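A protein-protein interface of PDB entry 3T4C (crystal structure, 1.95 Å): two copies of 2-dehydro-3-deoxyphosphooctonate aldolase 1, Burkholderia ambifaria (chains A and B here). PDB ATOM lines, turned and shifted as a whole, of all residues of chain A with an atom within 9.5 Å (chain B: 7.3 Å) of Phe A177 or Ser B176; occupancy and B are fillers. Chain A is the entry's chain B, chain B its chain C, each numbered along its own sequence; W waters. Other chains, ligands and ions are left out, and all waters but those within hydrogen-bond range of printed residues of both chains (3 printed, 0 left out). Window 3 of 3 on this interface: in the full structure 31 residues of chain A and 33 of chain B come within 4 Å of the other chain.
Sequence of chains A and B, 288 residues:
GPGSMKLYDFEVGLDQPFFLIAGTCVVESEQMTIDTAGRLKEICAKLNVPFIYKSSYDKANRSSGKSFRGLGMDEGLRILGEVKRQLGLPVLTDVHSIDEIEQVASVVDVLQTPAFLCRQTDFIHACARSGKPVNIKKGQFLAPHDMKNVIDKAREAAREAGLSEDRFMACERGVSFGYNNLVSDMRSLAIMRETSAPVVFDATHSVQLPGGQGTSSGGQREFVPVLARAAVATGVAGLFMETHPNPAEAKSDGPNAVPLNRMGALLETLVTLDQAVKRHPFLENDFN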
ATOM      1  N   GLN A 140      34.335 -15.438 -12.716  1.00  0.00           N
ATOM      2  CA  GLN A 140      33.446 -16.532 -12.257  1.00  0.00           C
ATOM      3  C   GLN A 140      31.975 -16.307 -12.559  1.00  0.00           C
ATOM      4  O   GLN A 140      31.182 -17.218 -12.419  1.00  0.00           O
ATOM      5  CB  GLN A 140      33.709 -16.848 -10.770  1.00  0.00           C
ATOM      6  CG  GLN A 140      33.654 -15.674  -9.824  1.00  0.00           C
ATOM      7  CD  GLN A 140      35.046 -14.998  -9.661  1.00  0.00           C
ATOM      8  OE1 GLN A 140      35.580 -14.403 -10.596  1.00  0.00           O
ATOM      9  NE2 GLN A 140      35.608 -15.074  -8.439  1.00  0.00           N
ATOM     10  N   PHE A 141      31.652 -15.095 -13.058  1.00  0.00           N
ATOM     11  CA  PHE A 141      30.318 -14.668 -13.473  1.00  0.00           C
ATOM     12  C   PHE A 141      30.131 -14.649 -15.009  1.00  0.00           C
ATOM     13  O   PHE A 141      29.074 -14.231 -15.505  1.00  0.00           O
ATOM     14  CB  PHE A 141      29.991 -13.265 -12.900  1.00  0.00           C
ATOM     15  CG  PHE A 141      31.117 -12.271 -13.070  1.00  0.00           C
ATOM     16  CD1 PHE A 141      31.238 -11.517 -14.238  1.00  0.00           C
ATOM     17  CD2 PHE A 141      32.073 -12.112 -12.079  1.00  0.00           C
ATOM     18  CE1 PHE A 141      32.291 -10.610 -14.392  1.00  0.00           C
ATOM     19  CE2 PHE A 141      33.129 -11.243 -12.251  1.00  0.00           C
ATOM     20  CZ  PHE A 141      33.238 -10.489 -13.406  1.00  0.00           C
ATOM     21  N   GLY A 174      37.122 -21.462 -12.818  1.00  0.00           N
ATOM     22  CA  GLY A 174      35.846 -21.819 -12.229  1.00  0.00           C
ATOM     23  C   GLY A 174      34.734 -20.832 -12.468  1.00  0.00           C
ATOM     24  O   GLY A 174      34.961 -19.626 -12.763  1.00  0.00           O
ATOM     25  N   VAL A 175      33.513 -21.332 -12.323  1.00  0.00           N
ATOM     26  CA  VAL A 175      32.307 -20.480 -12.421  1.00  0.00           C
ATOM     27  C   VAL A 175      31.495 -20.683 -11.149  1.00  0.00           C
ATOM     28  O   VAL A 175      31.540 -21.751 -10.556  1.00  0.00           O
ATOM     29  CB  VAL A 175      31.489 -20.791 -13.714  1.00  0.00           C
ATOM     30  CG1 VAL A 175      30.826 -22.167 -13.698  1.00  0.00           C
ATOM     31  CG2 VAL A 175      30.402 -19.780 -13.909  1.00  0.00           C
ATOM     32  N   SER A 176      30.734 -19.656 -10.746  1.00  0.00           N
ATOM     33  CA  SER A 176      30.018 -19.695  -9.481  1.00  0.00           C
ATOM     34  C   SER A 176      28.966 -20.767  -9.538  1.00  0.00           C
ATOM     35  O   SER A 176      28.239 -20.901 -10.536  1.00  0.00           O
ATOM     36  CB  SER A 176      29.396 -18.338  -9.116  1.00  0.00           C
ATOM     37  OG  SER A 176      30.406 -17.368  -9.073  1.00  0.00           O
ATOM     38  N   PHE A 177      28.864 -21.522  -8.452  1.00  0.00           N
ATOM     39  CA  PHE A 177      27.929 -22.636  -8.392  1.00  0.00           C
ATOM     40  C   PHE A 177      27.255 -22.594  -7.036  1.00  0.00           C
ATOM     41  O   PHE A 177      27.764 -23.114  -6.055  1.00  0.00           O
ATOM     42  CB  PHE A 177      28.673 -23.989  -8.576  1.00  0.00           C
ATOM     43  CG  PHE A 177      27.729 -25.193  -8.648  1.00  0.00           C
ATOM     44  CD1 PHE A 177      26.706 -25.231  -9.575  1.00  0.00           C
ATOM     45  CD2 PHE A 177      27.835 -26.259  -7.757  1.00  0.00           C
ATOM     46  CE1 PHE A 177      25.822 -26.325  -9.639  1.00  0.00           C
ATOM     47  CE2 PHE A 177      26.962 -27.345  -7.823  1.00  0.00           C
ATOM     48  CZ  PHE A 177      25.963 -27.366  -8.767  1.00  0.00           C
ATOM     49  N   GLY A 178      26.091 -21.969  -6.985  1.00  0.00           N
ATOM     50  CA  GLY A 178      25.466 -21.659  -5.693  1.00  0.00           C
ATOM     51  C   GLY A 178      26.322 -20.703  -4.905  1.00  0.00           C
ATOM     52  O   GLY A 178      27.012 -19.846  -5.494  1.00  0.00           O
ATOM     53  N   TYR A 179      26.263 -20.813  -3.581  1.00  0.00           N
ATOM     54  CA  TYR A 179      27.045 -19.960  -2.676  1.00  0.00           C
ATOM     55  C   TYR A 179      28.332 -20.718  -2.259  1.00  0.00           C
ATOM     56  O   TYR A 179      28.284 -21.934  -2.019  1.00  0.00           O
ATOM     57  CB  TYR A 179      26.242 -19.631  -1.424  1.00  0.00           C
ATOM     58  CG  TYR A 179      25.035 -18.744  -1.659  1.00  0.00           C
ATOM     59  CD1 TYR A 179      25.125 -17.606  -2.442  1.00  0.00           C
ATOM     60  CD2 TYR A 179      23.811 -19.031  -1.067  1.00  0.00           C
ATOM     61  CE1 TYR A 179      24.021 -16.802  -2.675  1.00  0.00           C
ATOM     62  CE2 TYR A 179      22.683 -18.221  -1.283  1.00  0.00           C
ATOM     63  CZ  TYR A 179      22.816 -17.100  -2.090  1.00  0.00           C
ATOM     64  OH  TYR A 179      21.747 -16.282  -2.290  1.00  0.00           O
ATOM     65  N   ASN A 180      29.455 -20.011  -2.223  1.00  0.00           N
ATOM     66  CA  ASN A 180      30.694 -20.518  -1.675  1.00  0.00           C
ATOM     67  C   ASN A 180      31.172 -21.796  -2.356  1.00  0.00           C
ATOM     68  O   ASN A 180      31.672 -22.704  -1.697  1.00  0.00           O
ATOM     69  CB  ASN A 180      30.588 -20.760  -0.171  1.00  0.00           C
ATOM     70  CG  ASN A 180      30.115 -19.523   0.582  1.00  0.00           C
ATOM     71  OD1 ASN A 180      30.762 -18.486   0.537  1.00  0.00           O
ATOM     72  ND2 ASN A 180      28.972 -19.631   1.242  1.00  0.00           N
ATOM     73  N   ASN A 181      31.060 -21.839  -3.678  1.00  0.00           N
ATOM     74  CA  ASN A 181      31.474 -23.014  -4.438  1.00  0.00           C
ATOM     75  C   ASN A 181      31.675 -22.593  -5.873  1.00  0.00           C
ATOM     76  O   ASN A 181      30.950 -21.745  -6.369  1.00  0.00           O
ATOM     77  CB  ASN A 181      30.432 -24.127  -4.386  1.00  0.00           C
ATOM     78  CG  ASN A 181      31.066 -25.512  -4.546  1.00  0.00           C
ATOM     79  OD1 ASN A 181      32.283 -25.633  -4.721  1.00  0.00           O
ATOM     80  ND2 ASN A 181      30.273 -26.536  -4.433  1.00  0.00           N
ATOM     81  N   LEU A 182      32.698 -23.150  -6.491  1.00  0.00           N
ATOM     82  CA  LEU A 182      32.963 -22.974  -7.891  1.00  0.00           C
ATOM     83  C   LEU A 182      32.794 -24.361  -8.533  1.00  0.00           C
ATOM     84  O   LEU A 182      32.878 -25.419  -7.850  1.00  0.00           O
ATOM     85  CB  LEU A 182      34.392 -22.420  -8.114  1.00  0.00           C
ATOM     86  CG  LEU A 182      34.698 -20.999  -7.648  1.00  0.00           C
ATOM     87  CD1 LEU A 182      36.198 -20.662  -7.790  1.00  0.00           C
ATOM     88  CD2 LEU A 182      33.857 -20.013  -8.423  1.00  0.00           C
ATOM     89  N   VAL A 183      32.441 -24.385  -9.801  1.00  0.00           N
ATOM     90  CA  VAL A 183      32.443 -25.649 -10.556  1.00  0.00           C
ATOM     91  C   VAL A 183      33.298 -25.420 -11.800  1.00  0.00           C
ATOM     92  O   VAL A 183      33.349 -24.309 -12.338  1.00  0.00           O
ATOM     93  CB  VAL A 183      31.005 -26.141 -10.883  1.00  0.00           C
ATOM     94  CG1 VAL A 183      30.300 -25.153 -11.840  1.00  0.00           C
ATOM     95  CG2 VAL A 183      31.041 -27.549 -11.483  1.00  0.00           C
ATOM     96  N   SER A 184      33.987 -26.492 -12.220  1.00  0.00           N
ATOM     97  CA  SER A 184      34.858 -26.460 -13.376  1.00  0.00           C
ATOM     98  C   SER A 184      34.175 -27.131 -14.566  1.00  0.00           C
ATOM     99  O   SER A 184      34.132 -28.360 -14.659  1.00  0.00           O
ATOM    100  CB  SER A 184      36.177 -27.161 -13.033  1.00  0.00           C
ATOM    101  OG  SER A 184      37.022 -26.308 -12.289  1.00  0.00           O
ATOM    102  N   ASP A 185      33.597 -26.327 -15.452  1.00  0.00           N
ATOM    103  CA  ASP A 185      32.852 -26.873 -16.595  1.00  0.00           C
ATOM    104  C   ASP A 185      33.866 -27.159 -17.695  1.00  0.00           C
ATOM    105  O   ASP A 185      34.343 -26.235 -18.316  1.00  0.00           O
ATOM    106  CB  ASP A 185      31.833 -25.850 -17.059  1.00  0.00           C
ATOM    107  CG  ASP A 185      30.910 -26.367 -18.133  1.00  0.00           C
ATOM    108  OD1 ASP A 185      31.131 -27.486 -18.688  1.00  0.00           O
ATOM    109  OD2 ASP A 185      29.908 -25.616 -18.398  1.00  0.00           O
ATOM    110  N   ARG A 187      33.493 -28.141 -20.606  1.00  0.00           N
ATOM    111  CA  ARG A 187      33.051 -27.578 -21.886  1.00  0.00           C
ATOM    112  C   ARG A 187      33.725 -26.209 -22.161  1.00  0.00           C
ATOM    113  O   ARG A 187      33.970 -25.844 -23.318  1.00  0.00           O
ATOM    114  CB  ARG A 187      31.517 -27.417 -21.911  1.00  0.00           C
ATOM    115  CG  ARG A 187      30.754 -28.740 -21.783  1.00  0.00           C
ATOM    116  CD  ARG A 187      29.260 -28.557 -21.727  1.00  0.00           C
ATOM    117  NE  ARG A 187      28.859 -27.760 -20.589  1.00  0.00           N
ATOM    118  CZ  ARG A 187      27.605 -27.556 -20.203  1.00  0.00           C
ATOM    119  NH1 ARG A 187      26.585 -28.055 -20.899  1.00  0.00           N
ATOM    120  NH2 ARG A 187      27.373 -26.836 -19.114  1.00  0.00           N
ATOM    121  N   SER A 206      40.357 -23.144  -9.076  1.00  0.00           N
ATOM    122  CA  SER A 206      39.096 -23.784  -9.520  1.00  0.00           C
ATOM    123  C   SER A 206      38.435 -24.629  -8.408  1.00  0.00           C
ATOM    124  O   SER A 206      37.217 -24.820  -8.417  1.00  0.00           O
ATOM    125  CB  SER A 206      39.328 -24.646 -10.784  1.00  0.00           C
ATOM    126  OG  SER A 206      39.474 -23.838 -11.966  1.00  0.00           O
ATOM    127  N   GLN A 208      38.804 -23.876  -5.093  1.00  0.00           N
ATOM    128  CA  GLN A 208      38.652 -23.054  -3.892  1.00  0.00           C
ATOM    129  C   GLN A 208      37.180 -22.807  -3.524  1.00  0.00           C
ATOM    130  O   GLN A 208      36.305 -22.727  -4.399  1.00  0.00           O
ATOM    131  CB  GLN A 208      39.456 -21.742  -4.056  1.00  0.00           C
ATOM    132  CG  GLN A 208      38.790 -20.437  -3.645  1.00  0.00           C
ATOM    133  CD  GLN A 208      39.390 -19.257  -4.390  1.00  0.00           C
ATOM    134  OE1 GLN A 208      40.514 -18.829  -4.114  1.00  0.00           O
ATOM    135  NE2 GLN A 208      38.656 -18.757  -5.367  1.00  0.00           N
ATOM    136  N   LEU A 209      36.895 -22.728  -2.225  1.00  0.00           N
ATOM    137  CA  LEU A 209      35.536 -22.380  -1.790  1.00  0.00           C
ATOM    138  C   LEU A 209      35.539 -20.873  -1.536  1.00  0.00           C
ATOM    139  O   LEU A 209      36.136 -20.425  -0.569  1.00  0.00           O
ATOM    140  CB  LEU A 209      35.120 -23.168  -0.533  1.00  0.00           C
ATOM    141  CG  LEU A 209      34.998 -24.704  -0.643  1.00  0.00           C
ATOM    142  CD1 LEU A 209      34.332 -25.264   0.622  1.00  0.00           C
ATOM    143  CD2 LEU A 209      34.233 -25.170  -1.895  1.00  0.00           C
ATOM    144  N   PRO A 210      34.918 -20.077  -2.426  1.00  0.00           N
ATOM    145  CA  PRO A 210      34.876 -18.615  -2.184  1.00  0.00           C
ATOM    146  C   PRO A 210      34.376 -18.268  -0.784  1.00  0.00           C
ATOM    147  O   PRO A 210      33.438 -18.914  -0.314  1.00  0.00           O
ATOM    148  CB  PRO A 210      33.874 -18.093  -3.237  1.00  0.00           C
ATOM    149  CG  PRO A 210      33.487 -19.250  -4.093  1.00  0.00           C
ATOM    150  CD  PRO A 210      34.271 -20.457  -3.695  1.00  0.00           C
ATOM    151  N   GLY B 139      20.525 -38.369  -9.112  1.00  0.00           N
ATOM    152  CA  GLY B 139      19.630 -37.263  -9.483  1.00  0.00           C
ATOM    153  C   GLY B 139      20.401 -35.975  -9.711  1.00  0.00           C
ATOM    154  O   GLY B 139      21.402 -35.684  -9.036  1.00  0.00           O
ATOM    155  N   GLN B 140      19.888 -35.166 -10.601  1.00  0.00           N
ATOM    156  CA  GLN B 140      20.564 -33.892 -10.902  1.00  0.00           C
ATOM    157  C   GLN B 140      20.419 -32.866  -9.780  1.00  0.00           C
ATOM    158  O   GLN B 140      21.009 -31.797  -9.868  1.00  0.00           O
ATOM    159  CB  GLN B 140      20.064 -33.294 -12.205  1.00  0.00           C
ATOM    160  CG  GLN B 140      18.582 -33.280 -12.384  1.00  0.00           C
ATOM    161  CD  GLN B 140      18.004 -34.530 -13.077  1.00  0.00           C
ATOM    162  OE1 GLN B 140      18.069 -35.687 -12.561  1.00  0.00           O
ATOM    163  NE2 GLN B 140      17.395 -34.288 -14.250  1.00  0.00           N
ATOM    164  N   PHE B 141      19.571 -33.189  -8.799  1.00  0.00           N
ATOM    165  CA  PHE B 141      19.339 -32.405  -7.591  1.00  0.00           C
ATOM    166  C   PHE B 141      20.179 -32.864  -6.396  1.00  0.00           C
ATOM    167  O   PHE B 141      20.122 -32.240  -5.329  1.00  0.00           O
ATOM    168  CB  PHE B 141      17.825 -32.404  -7.204  1.00  0.00           C
ATOM    169  CG  PHE B 141      17.182 -33.790  -7.196  1.00  0.00           C
ATOM    170  CD1 PHE B 141      16.623 -34.311  -8.342  1.00  0.00           C
ATOM    171  CD2 PHE B 141      17.140 -34.552  -6.031  1.00  0.00           C
ATOM    172  CE1 PHE B 141      16.044 -35.586  -8.359  1.00  0.00           C
ATOM    173  CE2 PHE B 141      16.508 -35.798  -6.008  1.00  0.00           C
ATOM    174  CZ  PHE B 141      15.994 -36.338  -7.206  1.00  0.00           C
ATOM    175  N   LEU B 142      20.910 -33.962  -6.538  1.00  0.00           N
ATOM    176  CA  LEU B 142      21.725 -34.506  -5.432  1.00  0.00           C
ATOM    177  C   LEU B 142      23.140 -33.887  -5.407  1.00  0.00           C
ATOM    178  O   LEU B 142      23.627 -33.401  -6.419  1.00  0.00           O
ATOM    179  CB  LEU B 142      21.844 -36.014  -5.615  1.00  0.00           C
ATOM    180  CG  LEU B 142      20.995 -36.869  -4.665  1.00  0.00           C
ATOM    181  CD1 LEU B 142      19.584 -36.380  -4.483  1.00  0.00           C
ATOM    182  CD2 LEU B 142      21.152 -38.354  -4.973  1.00  0.00           C
ATOM    183  N   PRO B 144      27.115 -34.967  -4.595  1.00  0.00           N
ATOM    184  CA  PRO B 144      27.778 -36.260  -4.725  1.00  0.00           C
ATOM    185  C   PRO B 144      27.807 -37.078  -3.453  1.00  0.00           C
ATOM    186  O   PRO B 144      27.628 -38.298  -3.564  1.00  0.00           O
ATOM    187  CB  PRO B 144      29.185 -35.901  -5.134  1.00  0.00           C
ATOM    188  CG  PRO B 144      29.059 -34.551  -5.802  1.00  0.00           C
ATOM    189  CD  PRO B 144      27.943 -33.861  -5.088  1.00  0.00           C
ATOM    190  N   GLY B 174      25.262 -35.553 -14.505  1.00  0.00           N
ATOM    191  CA  GLY B 174      25.066 -34.114 -14.435  1.00  0.00           C
ATOM    192  C   GLY B 174      24.336 -33.601 -13.204  1.00  0.00           C
ATOM    193  O   GLY B 174      23.557 -34.337 -12.562  1.00  0.00           O
ATOM    194  N   VAL B 175      24.599 -32.350 -12.862  1.00  0.00           N
ATOM    195  CA  VAL B 175      23.870 -31.654 -11.799  1.00  0.00           C
ATOM    196  C   VAL B 175      23.296 -30.375 -12.419  1.00  0.00           C
ATOM    197  O   VAL B 175      23.904 -29.782 -13.327  1.00  0.00           O
ATOM    198  CB  VAL B 175      24.766 -31.367 -10.570  1.00  0.00           C
ATOM    199  CG1 VAL B 175      25.968 -30.458 -10.914  1.00  0.00           C
ATOM    200  CG2 VAL B 175      24.014 -30.660  -9.438  1.00  0.00           C
ATOM    201  N   SER B 176      22.094 -30.020 -11.998  1.00  0.00           N
ATOM    202  CA  SER B 176      21.456 -28.803 -12.404  1.00  0.00           C
ATOM    203  C   SER B 176      22.331 -27.555 -12.265  1.00  0.00           C
ATOM    204  O   SER B 176      22.834 -27.243 -11.199  1.00  0.00           O
ATOM    205  CB  SER B 176      20.149 -28.626 -11.649  1.00  0.00           C
ATOM    206  OG  SER B 176      19.267 -29.712 -11.978  1.00  0.00           O
ATOM    207  N   PHE B 177      22.427 -26.794 -13.351  1.00  0.00           N
ATOM    208  CA  PHE B 177      23.246 -25.613 -13.348  1.00  0.00           C
ATOM    209  C   PHE B 177      22.415 -24.442 -13.854  1.00  0.00           C
ATOM    210  O   PHE B 177      22.332 -24.225 -15.056  1.00  0.00           O
ATOM    211  CB  PHE B 177      24.484 -25.802 -14.221  1.00  0.00           C
ATOM    212  CG  PHE B 177      25.442 -24.643 -14.170  1.00  0.00           C
ATOM    213  CD1 PHE B 177      26.026 -24.272 -12.973  1.00  0.00           C
ATOM    214  CD2 PHE B 177      25.759 -23.922 -15.285  1.00  0.00           C
ATOM    215  CE1 PHE B 177      26.936 -23.203 -12.887  1.00  0.00           C
ATOM    216  CE2 PHE B 177      26.646 -22.844 -15.224  1.00  0.00           C
ATOM    217  CZ  PHE B 177      27.240 -22.482 -14.024  1.00  0.00           C
ATOM    218  N   GLY B 178      21.826 -23.681 -12.949  1.00  0.00           N
ATOM    219  CA  GLY B 178      20.812 -22.693 -13.334  1.00  0.00           C
ATOM    220  C   GLY B 178      19.636 -23.376 -14.037  1.00  0.00           C
ATOM    221  O   GLY B 178      19.306 -24.520 -13.698  1.00  0.00           O
ATOM    222  N   TYR B 179      19.000 -22.698 -14.990  1.00  0.00           N
ATOM    223  CA  TYR B 179      17.848 -23.278 -15.735  1.00  0.00           C
ATOM    224  C   TYR B 179      18.301 -23.908 -17.051  1.00  0.00           C
ATOM    225  O   TYR B 179      19.160 -23.336 -17.752  1.00  0.00           O
ATOM    226  CB  TYR B 179      16.851 -22.184 -16.112  1.00  0.00           C
ATOM    227  CG  TYR B 179      16.110 -21.599 -14.914  1.00  0.00           C
ATOM    228  CD1 TYR B 179      15.469 -22.441 -13.985  1.00  0.00           C
ATOM    229  CD2 TYR B 179      16.042 -20.231 -14.718  1.00  0.00           C
ATOM    230  CE1 TYR B 179      14.818 -21.912 -12.879  1.00  0.00           C
ATOM    231  CE2 TYR B 179      15.339 -19.697 -13.612  1.00  0.00           C
ATOM    232  CZ  TYR B 179      14.750 -20.566 -12.703  1.00  0.00           C
ATOM    233  OH  TYR B 179      14.115 -20.061 -11.615  1.00  0.00           O
ATOM    234  N   ASN B 180      17.733 -25.049 -17.397  1.00  0.00           N
ATOM    235  CA  ASN B 180      17.970 -25.658 -18.723  1.00  0.00           C
ATOM    236  C   ASN B 180      19.448 -25.911 -19.032  1.00  0.00           C
ATOM    237  O   ASN B 180      19.893 -25.749 -20.172  1.00  0.00           O
ATOM    238  CB  ASN B 180      17.371 -24.811 -19.825  1.00  0.00           C
ATOM    239  CG  ASN B 180      15.884 -24.612 -19.637  1.00  0.00           C
ATOM    240  OD1 ASN B 180      15.150 -25.580 -19.472  1.00  0.00           O
ATOM    241  ND2 ASN B 180      15.460 -23.383 -19.611  1.00  0.00           N
ATOM    242  N   ASN B 181      20.195 -26.336 -18.032  1.00  0.00           N
ATOM    243  CA  ASN B 181      21.627 -26.682 -18.254  1.00  0.00           C
ATOM    244  C   ASN B 181      22.063 -27.632 -17.135  1.00  0.00           C
ATOM    245  O   ASN B 181      21.575 -27.512 -15.989  1.00  0.00           O
ATOM    246  CB  ASN B 181      22.494 -25.418 -18.309  1.00  0.00           C
ATOM    247  CG  ASN B 181      23.775 -25.606 -19.137  1.00  0.00           C
ATOM    248  OD1 ASN B 181      24.195 -26.735 -19.412  1.00  0.00           O
ATOM    249  ND2 ASN B 181      24.356 -24.528 -19.573  1.00  0.00           N
ATOM    250  N   LEU B 182      22.931 -28.576 -17.488  1.00  0.00           N
ATOM    251  CA  LEU B 182      23.596 -29.443 -16.556  1.00  0.00           C
ATOM    252  C   LEU B 182      25.104 -29.187 -16.687  1.00  0.00           C
ATOM    253  O   LEU B 182      25.623 -28.933 -17.819  1.00  0.00           O
ATOM    254  CB  LEU B 182      23.340 -30.888 -16.887  1.00  0.00           C
ATOM    255  CG  LEU B 182      21.894 -31.376 -16.886  1.00  0.00           C
ATOM    256  CD1 LEU B 182      21.844 -32.794 -17.479  1.00  0.00           C
ATOM    257  CD2 LEU B 182      21.309 -31.326 -15.480  1.00  0.00           C
ATOM    258  N   VAL B 183      25.800 -29.274 -15.544  1.00  0.00           N
ATOM    259  CA  VAL B 183      27.240 -29.231 -15.497  1.00  0.00           C
ATOM    260  C   VAL B 183      27.757 -30.559 -14.966  1.00  0.00           C
ATOM    261  O   VAL B 183      27.142 -31.187 -14.098  1.00  0.00           O
ATOM    262  CB  VAL B 183      27.756 -28.003 -14.659  1.00  0.00           C
ATOM    263  CG1 VAL B 183      27.463 -28.178 -13.172  1.00  0.00           C
ATOM    264  CG2 VAL B 183      29.265 -27.753 -14.895  1.00  0.00           C
ATOM    265  N   ASP B 185      30.459 -32.046 -12.774  1.00  0.00           N
ATOM    266  CA  ASP B 185      31.472 -31.656 -11.769  1.00  0.00           C
ATOM    267  C   ASP B 185      32.370 -32.869 -11.593  1.00  0.00           C
ATOM    268  O   ASP B 185      31.943 -33.857 -11.021  1.00  0.00           O
ATOM    269  CB  ASP B 185      30.755 -31.337 -10.459  1.00  0.00           C
ATOM    270  CG  ASP B 185      31.676 -30.807  -9.403  1.00  0.00           C
ATOM    271  OD1 ASP B 185      32.916 -30.838  -9.624  1.00  0.00           O
ATOM    272  OD2 ASP B 185      31.133 -30.356  -8.337  1.00  0.00           O
ATOM    273  N   ARG B 187      34.643 -33.441  -9.755  1.00  0.00           N
ATOM    274  CA  ARG B 187      34.840 -33.763  -8.296  1.00  0.00           C
ATOM    275  C   ARG B 187      33.917 -34.869  -7.842  1.00  0.00           C
ATOM    276  O   ARG B 187      34.300 -35.672  -6.961  1.00  0.00           O
ATOM    277  CB  ARG B 187      34.620 -32.533  -7.388  1.00  0.00           C
ATOM    278  CG  ARG B 187      35.608 -31.395  -7.659  1.00  0.00           C
ATOM    279  CD  ARG B 187      35.334 -30.172  -6.798  1.00  0.00           C
ATOM    280  NE  ARG B 187      34.019 -29.619  -7.081  1.00  0.00           N
ATOM    281  CZ  ARG B 187      33.551 -28.439  -6.678  1.00  0.00           C
ATOM    282  NH1 ARG B 187      34.230 -27.634  -5.883  1.00  0.00           N
ATOM    283  NH2 ARG B 187      32.326 -28.096  -7.044  1.00  0.00           N
ATOM    284  N   PRO B 210      18.356 -29.776 -20.481  1.00  0.00           N
ATOM    285  CA  PRO B 210      16.987 -30.151 -20.016  1.00  0.00           C
ATOM    286  C   PRO B 210      15.809 -29.417 -20.674  1.00  0.00           C
ATOM    287  O   PRO B 210      15.776 -28.184 -20.659  1.00  0.00           O
ATOM    288  CB  PRO B 210      17.021 -29.801 -18.517  1.00  0.00           C
ATOM    289  CG  PRO B 210      18.455 -29.844 -18.122  1.00  0.00           C
ATOM    290  CD  PRO B 210      19.299 -29.643 -19.351  1.00  0.00           C
HETATM  291  O   HOH W   1      35.536 -27.002  -8.776  1.00  0.00           O
HETATM  292  O   HOH W   2      27.527 -30.513 -19.005  1.00  0.00           O
HETATM  293  O   HOH W   3      34.428 -28.807 -10.531  1.00  0.00           O
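The backbone NH (N) of Ser A176 sits at hydrogen-bond distance from the backbone carbonyl oxygen (O) of Gln A140, 3.0 Å away. The backbone carbonyl oxygen (O) of Gln B140 is in hydrogen-bond range of the backbone NH (N) of Ser B176 (3.0 Å). OD2 of Asp B185 is in salt-bridge range of NH2 of Arg B187 (2.9 Å). The backbone NH of Val A183 lies within hydrogen-bond range of the backbone carbonyl oxygen of Val A175. The side-chain carboxylate of Asp A185 is in salt-bridge range of the guanidinium group of Arg A187, at 2.9 Å. The backbone carbonyl oxygen (O) of Val B175 lies within hydrogen-bond range of the backbone NH (N) of Val B183 (3.0 Å).
Water W3 bridges OD1 of Asp B185 (2.7 Å) and N of Ser A184 (2.9 Å). Water W2 lies within hydrogen-bond range of the backbone carbonyl oxygen (O) of Leu B182 (2.7 Å) and the guanidinium group (NH1) of Arg A187 (3.2 Å). Water W1 lies within hydrogen-bond range of O of Ser A206, O of Leu A182 and NH1 of Arg B187.
Ser A176 touches Phe B177, and with the chains exchanged Phe A177 touches Ser B176. Leu A182 touches Arg B187, and with the chains exchanged Arg A187 touches Leu B182. Val B183 touches its own counterpart, Val A183. Val A183 touches Asp B185, and with the chains exchanged Asp A185 touches Val B183. Of the 12 pairs that touch across the chains among the printed residues, 12 have their exchanged pair printed and touching as well.
Phe A177 touches just these residues of chain B: Val B175 (3.8 Å), Ser B176 (3.5 Å) and Phe B177 (3.6 Å). No residue of chain B comes within 4 Å of Gly A178. Printed residues of chain B within 4 Å of Val A183: Val B183 and Asp B185. Phe B141 touches none of the printed residues of chain A. Of chain A, only Phe A177 (3.5 Å) comes within 4 Å of Ser B176. No residue of chain A comes within 4 Å of Gly B178. Of the printed residues of chain A, Leu B182 touches Arg A187. Printed residues of chain A within 4 Å of Arg B187: Asn A181 and Leu A182. The nearest residue of chain A that does not touch Ser B176 is Gly A178 (7.5 Å).
Val A175 touches Phe B177 (CG1 to CZ, 3.6 Å). Phe B177 touches Ser A176. Val B175 touches Phe A177 (CG1 to CZ, 3.8 Å). Phe A177 touches Ser B176 (CE1 to O, 3.5 Å). CD1 of Phe A177 touches CD1 of Phe B177, at 3.6 Å. CG2 of Val A183 touches CG2 of Val B183, 3.9 Å away. CG2 of Val A183 touches CG of Asp B185, 3.9 Å away. Asp A185 touches Val B183.
Printed residues of chain A that touch a printed residue of chain B: Val A175, Ser A176, Phe A177, Asn A181, Leu A182, Val A183, Asp A185 and Arg A187. Hydrophobic or aromatic side chains of chain A that line the printed part of chain B: Val A175, Phe A177 and Val A183. Among the printed residues, no Asp or Glu carboxylate lies within 4 Å of a Lys or Arg side-chain nitrogen of the other chain.
NH2 of Arg A187 is in hydrogen-bond range of O of Leu B182, at 3.0 Å. O of Leu A182 lies within hydrogen-bond range of NH2 of Arg B187. OD1 of Asn A181 is in hydrogen-bond range of NH1 of Arg B187 (3.0 Å). The side-chain amide oxygen of Asn B181 is in hydrogen-bond range of the guanidinium group of Arg A187, 3.1 Å away.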
